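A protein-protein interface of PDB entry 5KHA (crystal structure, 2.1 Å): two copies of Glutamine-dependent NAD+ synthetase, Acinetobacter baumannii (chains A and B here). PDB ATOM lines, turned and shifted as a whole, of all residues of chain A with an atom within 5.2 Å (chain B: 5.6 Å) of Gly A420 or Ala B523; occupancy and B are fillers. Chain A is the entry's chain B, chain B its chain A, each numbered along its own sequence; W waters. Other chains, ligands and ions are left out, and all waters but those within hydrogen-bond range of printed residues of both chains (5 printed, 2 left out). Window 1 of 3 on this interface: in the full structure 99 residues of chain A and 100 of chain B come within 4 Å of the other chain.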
ATOM      1  N   VAL A 398       5.315   6.416  -9.744  1.00  0.00           N
ATOM      2  CA  VAL A 398       5.389   4.991  -9.438  1.00  0.00           C
ATOM      3  C   VAL A 398       4.689   4.715  -8.111  1.00  0.00           C
ATOM      4  O   VAL A 398       5.018   5.316  -7.079  1.00  0.00           O
ATOM      5  CB  VAL A 398       6.843   4.501  -9.386  1.00  0.00           C
ATOM      6  CG1 VAL A 398       6.858   3.021  -8.990  1.00  0.00           C
ATOM      7  CG2 VAL A 398       7.597   4.761 -10.727  1.00  0.00           C
ATOM      8  N   LEU A 399       3.734   3.791  -8.131  1.00  0.00           N
ATOM      9  CA  LEU A 399       3.048   3.341  -6.926  1.00  0.00           C
ATOM     10  C   LEU A 399       3.739   2.081  -6.424  1.00  0.00           C
ATOM     11  O   LEU A 399       3.755   1.059  -7.125  1.00  0.00           O
ATOM     12  CB  LEU A 399       1.574   3.052  -7.221  1.00  0.00           C
ATOM     13  CG  LEU A 399       0.749   4.245  -7.706  1.00  0.00           C
ATOM     14  CD1 LEU A 399      -0.677   3.815  -8.052  1.00  0.00           C
ATOM     15  CD2 LEU A 399       0.759   5.392  -6.650  1.00  0.00           C
ATOM     16  N   SER A 400       4.342   2.150  -5.243  1.00  0.00           N
ATOM     17  CA  SER A 400       4.884   0.957  -4.608  1.00  0.00           C
ATOM     18  C   SER A 400       3.749   0.128  -4.012  1.00  0.00           C
ATOM     19  O   SER A 400       2.734   0.668  -3.563  1.00  0.00           O
ATOM     20  CB  SER A 400       5.888   1.333  -3.521  1.00  0.00           C
ATOM     21  OG  SER A 400       6.271   0.192  -2.775  1.00  0.00           O
ATOM     22  N   MET A 418      10.507  -1.710  -2.944  1.00  0.00           N
ATOM     23  CA  MET A 418      10.194  -0.477  -2.227  1.00  0.00           C
ATOM     24  C   MET A 418      10.170   0.745  -3.135  1.00  0.00           C
ATOM     25  O   MET A 418       9.725   1.812  -2.699  1.00  0.00           O
ATOM     26  CB  MET A 418      11.194  -0.258  -1.084  1.00  0.00           C
ATOM     27  CG  MET A 418      10.965  -1.247   0.046  1.00  0.00           C
ATOM     28  SD  MET A 418      12.166  -1.110   1.372  1.00  0.00           S
ATOM     29  CE  MET A 418      11.846   0.563   1.950  1.00  0.00           C
ATOM     30  N   VAL A 419      10.609   0.605  -4.390  1.00  0.00           N
ATOM     31  CA  VAL A 419      10.675   1.738  -5.308  1.00  0.00           C
ATOM     32  C   VAL A 419       9.289   2.349  -5.516  1.00  0.00           C
ATOM     33  O   VAL A 419       8.318   1.648  -5.843  1.00  0.00           O
ATOM     34  CB  VAL A 419      11.301   1.286  -6.638  1.00  0.00           C
ATOM     35  CG1 VAL A 419      11.022   2.307  -7.742  1.00  0.00           C
ATOM     36  CG2 VAL A 419      12.784   1.097  -6.453  1.00  0.00           C
ATOM     37  N   GLY A 420       9.202   3.668  -5.380  1.00  0.00           N
ATOM     38  CA  GLY A 420       7.955   4.362  -5.623  1.00  0.00           C
ATOM     39  C   GLY A 420       7.926   5.725  -4.966  1.00  0.00           C
ATOM     40  O   GLY A 420       8.740   6.062  -4.104  1.00  0.00           O
ATOM     41  N   GLY A 421       6.975   6.540  -5.414  1.00  0.00           N
ATOM     42  CA  GLY A 421       6.761   7.853  -4.833  1.00  0.00           C
ATOM     43  C   GLY A 421       5.562   7.879  -3.900  1.00  0.00           C
ATOM     44  O   GLY A 421       5.355   8.857  -3.172  1.00  0.00           O
ATOM     45  N   PHE A 422       4.750   6.824  -3.926  1.00  0.00           N
ATOM     46  CA  PHE A 422       3.585   6.722  -3.044  1.00  0.00           C
ATOM     47  C   PHE A 422       3.288   5.251  -2.828  1.00  0.00           C
ATOM     48  O   PHE A 422       3.219   4.484  -3.795  1.00  0.00           O
ATOM     49  CB  PHE A 422       2.363   7.405  -3.646  1.00  0.00           C
ATOM     50  CG  PHE A 422       1.250   7.671  -2.665  1.00  0.00           C
ATOM     51  CD1 PHE A 422       1.354   8.705  -1.740  1.00  0.00           C
ATOM     52  CD2 PHE A 422       0.082   6.912  -2.699  1.00  0.00           C
ATOM     53  CE1 PHE A 422       0.316   8.980  -0.843  1.00  0.00           C
ATOM     54  CE2 PHE A 422      -0.953   7.156  -1.810  1.00  0.00           C
ATOM     55  CZ  PHE A 422      -0.841   8.214  -0.881  1.00  0.00           C
ATOM     56  N   ALA A 423       3.133   4.874  -1.567  1.00  0.00           N
ATOM     57  CA  ALA A 423       2.960   3.495  -1.132  1.00  0.00           C
ATOM     58  C   ALA A 423       1.548   3.376  -0.555  1.00  0.00           C
ATOM     59  O   ALA A 423       1.328   3.596   0.634  1.00  0.00           O
ATOM     60  CB  ALA A 423       4.036   3.120  -0.112  1.00  0.00           C
ATOM     61  N   LYS A 426       1.032   0.919   2.480  1.00  0.00           N
ATOM     62  CA  LYS A 426       2.096   0.831   3.478  1.00  0.00           C
ATOM     63  C   LYS A 426       1.540   0.699   4.896  1.00  0.00           C
ATOM     64  O   LYS A 426       2.201   0.120   5.758  1.00  0.00           O
ATOM     65  CB  LYS A 426       3.056   2.033   3.376  1.00  0.00           C
ATOM     66  CG  LYS A 426       2.723   3.226   4.244  1.00  0.00           C
ATOM     67  CD  LYS A 426       3.806   4.356   4.106  1.00  0.00           C
ATOM     68  CE  LYS A 426       5.067   4.141   4.916  1.00  0.00           C
ATOM     69  NZ  LYS A 426       5.977   5.339   4.770  1.00  0.00           N
ATOM     70  N   GLN A 521      13.530   9.877   1.208  1.00  0.00           N
ATOM     71  CA  GLN A 521      13.900   8.492   0.941  1.00  0.00           C
ATOM     72  C   GLN A 521      15.397   8.241   1.079  1.00  0.00           C
ATOM     73  O   GLN A 521      15.827   7.093   0.984  1.00  0.00           O
ATOM     74  CB  GLN A 521      13.403   8.102  -0.461  1.00  0.00           C
ATOM     75  CG  GLN A 521      11.879   8.161  -0.596  1.00  0.00           C
ATOM     76  CD  GLN A 521      11.344   7.464  -1.857  1.00  0.00           C
ATOM     77  OE1 GLN A 521      11.927   6.506  -2.359  1.00  0.00           O
ATOM     78  NE2 GLN A 521      10.243   7.974  -2.382  1.00  0.00           N
ATOM     79  N   TYR B 415      17.500   5.847  -5.649  1.00  0.00           N
ATOM     80  CA  TYR B 415      17.950   4.471  -5.853  1.00  0.00           C
ATOM     81  C   TYR B 415      19.217   4.367  -6.704  1.00  0.00           C
ATOM     82  O   TYR B 415      19.552   3.272  -7.150  1.00  0.00           O
ATOM     83  CB  TYR B 415      16.836   3.603  -6.471  1.00  0.00           C
ATOM     84  CG  TYR B 415      15.464   4.081  -6.061  1.00  0.00           C
ATOM     85  CD1 TYR B 415      15.109   4.146  -4.714  1.00  0.00           C
ATOM     86  CD2 TYR B 415      14.534   4.477  -7.005  1.00  0.00           C
ATOM     87  CE1 TYR B 415      13.861   4.603  -4.321  1.00  0.00           C
ATOM     88  CE2 TYR B 415      13.275   4.919  -6.624  1.00  0.00           C
ATOM     89  CZ  TYR B 415      12.946   4.989  -5.272  1.00  0.00           C
ATOM     90  OH  TYR B 415      11.687   5.412  -4.877  1.00  0.00           O
ATOM     91  N   GLN B 521      13.463   4.587   4.566  1.00  0.00           N
ATOM     92  CA  GLN B 521      13.804   4.921   3.189  1.00  0.00           C
ATOM     93  C   GLN B 521      12.673   4.657   2.196  1.00  0.00           C
ATOM     94  O   GLN B 521      12.799   5.038   1.024  1.00  0.00           O
ATOM     95  CB  GLN B 521      15.068   4.164   2.777  1.00  0.00           C
ATOM     96  CG  GLN B 521      16.306   4.565   3.591  1.00  0.00           C
ATOM     97  CD  GLN B 521      17.607   4.141   2.919  1.00  0.00           C
ATOM     98  OE1 GLN B 521      17.689   4.060   1.694  1.00  0.00           O
ATOM     99  NE2 GLN B 521      18.625   3.868   3.719  1.00  0.00           N
ATOM    100  N   GLY B 522      11.559   4.055   2.640  1.00  0.00           N
ATOM    101  CA  GLY B 522      10.441   3.816   1.757  1.00  0.00           C
ATOM    102  C   GLY B 522       9.613   5.062   1.507  1.00  0.00           C
ATOM    103  O   GLY B 522       9.677   6.047   2.251  1.00  0.00           O
ATOM    104  N   ALA B 523       8.803   4.996   0.447  1.00  0.00           N
ATOM    105  CA  ALA B 523       7.955   6.115   0.065  1.00  0.00           C
ATOM    106  C   ALA B 523       6.885   6.386   1.124  1.00  0.00           C
ATOM    107  O   ALA B 523       6.490   5.503   1.891  1.00  0.00           O
ATOM    108  CB  ALA B 523       7.271   5.839  -1.278  1.00  0.00           C
ATOM    109  N   ILE B 524       6.396   7.634   1.143  1.00  0.00           N
ATOM    110  CA  ILE B 524       5.257   7.933   2.005  1.00  0.00           C
ATOM    111  C   ILE B 524       4.036   7.162   1.518  1.00  0.00           C
ATOM    112  O   ILE B 524       3.974   6.686   0.377  1.00  0.00           O
ATOM    113  CB  ILE B 524       4.954   9.439   2.075  1.00  0.00           C
ATOM    114  CG1 ILE B 524       5.295  10.104   0.754  1.00  0.00           C
ATOM    115  CG2 ILE B 524       5.670  10.088   3.242  1.00  0.00           C
ATOM    116  CD1 ILE B 524       4.160  10.137  -0.203  1.00  0.00           C
ATOM    117  N   GLY B 525       3.062   7.028   2.424  1.00  0.00           N
ATOM    118  CA  GLY B 525       1.819   6.339   2.187  1.00  0.00           C
ATOM    119  C   GLY B 525       0.793   6.731   3.232  1.00  0.00           C
ATOM    120  O   GLY B 525       1.133   7.310   4.261  1.00  0.00           O
HETATM  121  O   HOH W   1       8.144   2.156  -0.472  1.00  0.00           O
HETATM  122  O   HOH W   2      15.137   4.749  -0.901  1.00  0.00           O
HETATM  123  O   HOH W   3      18.207   6.108  -0.478  1.00  0.00           O
HETATM  124  O   HOH W   4       8.770   6.315   5.173  1.00  0.00           O
HETATM  125  O   HOH W   5       9.949   6.467  -7.060  1.00  0.00           O
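The backbone NH of Gly A420 is in hydrogen-bond range of the side-chain hydroxyl of Tyr B415 (3.1 Å).
OH of Tyr B415 lies within hydrogen-bond range of OE1 of Gln A521.
NZ of Lys A426 sits at hydrogen-bond distance from O of Ala B523 (2.9 Å).
The backbone NH (N) of Ala A423 lies within hydrogen-bond range of the backbone carbonyl oxygen (O) of Ile B524, 2.8 Å away.
N of Gly A421 is in hydrogen-bond range of O of Val A398, at 2.8 Å.
N of Ser A400 lies within hydrogen-bond range of O of Phe A422 (3.0 Å).
The backbone carbonyl oxygen of Gly A420 sits at hydrogen-bond distance from the side-chain amide nitrogen of Gln A521, 3.0 Å away.
Among the printed residues, merely in contact across the chains: Ala A423 with Gly B525 (3.2 Å), Gly A420 with Ala B523 (3.2 Å), Lys A426 with Gly B525 (3.2 Å), Phe A422 with Ile B524 (3.4 Å), Gly A421 with Ile B524 (3.4 Å), Gln A521 with Gln B521 (3.5 Å), Met A418 with Gly B522 (3.5 Å), Val A419 with Tyr B415 (3.6 Å), Gly A421 with Ala B523 (3.7 Å), Phe A422 with Ala B523 (3.8 Å), Gln A521 with Ala B523 (3.8 Å), Lys A426 with Ile B524 (3.8 Å) and Ala A423 with Ala B523 (3.96 Å).
Of chain A, only Gly A420, Gly A421, Phe A422, Ala A423, Lys A426 and Gln A521 come within 4 Å of Ala B523.
Printed residues of chain A within 4 Å of Tyr B415: Val A419, Gly A420 and Gln A521.
Of the printed residues of chain B, Gln A521 touches Tyr B415 (2.8 Å), Gln B521 (3.5 Å) and Ala B523 (3.8 Å).
The nearest printed residue of chain B that does not touch Gly A420 is Gly B522 (5.8 Å).
Of the 11 printed residues of chain A, 8 touch a printed residue of chain B.
Hydrophobic or aromatic side chains of chain A within 4 Å of the printed part of chain B: Met A418, Val A419, Phe A422 and Ala A423.
Hydrophobic or aromatic side chains of chain B within 4 Å of the printed part of chain A: Tyr B415, Ala B523 and Ile B524.
Along chain B the printed residues that touch a printed residue of chain A span positions 415 to 525.
Among the printed residues, no Asp or Glu carboxylate lies within 4 Å of a Lys or Arg side-chain nitrogen of the other chain.
Gln A521 touches its own counterpart, Gln B521.
Of the 17 pairs that touch across the chains among the printed residues, 1 has its exchanged pair printed and touching as well.
Water W1 bridges O of Met A418 (2.8 Å) and N of Ala B523 (3.1 Å).
Water W3 bridges the backbone carbonyl oxygen of Gln A521 (3.0 Å) and the side-chain amide oxygen of Gln B521 (3.0 Å).
Water W5 lies within hydrogen-bond range of the side-chain hydroxyl (OH) of Tyr B415, the backbone carbonyl oxygen (O) of Gly A420 and the backbone NH (N) of Gly A421.
Water W4 bridges NZ of Lys A426 (3.0 Å) and O of Gly B522 (3.1 Å).
Water W2 bridges the backbone carbonyl oxygen (O) of Gln B521 and the backbone carbonyl oxygen (O) of Gln A521.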
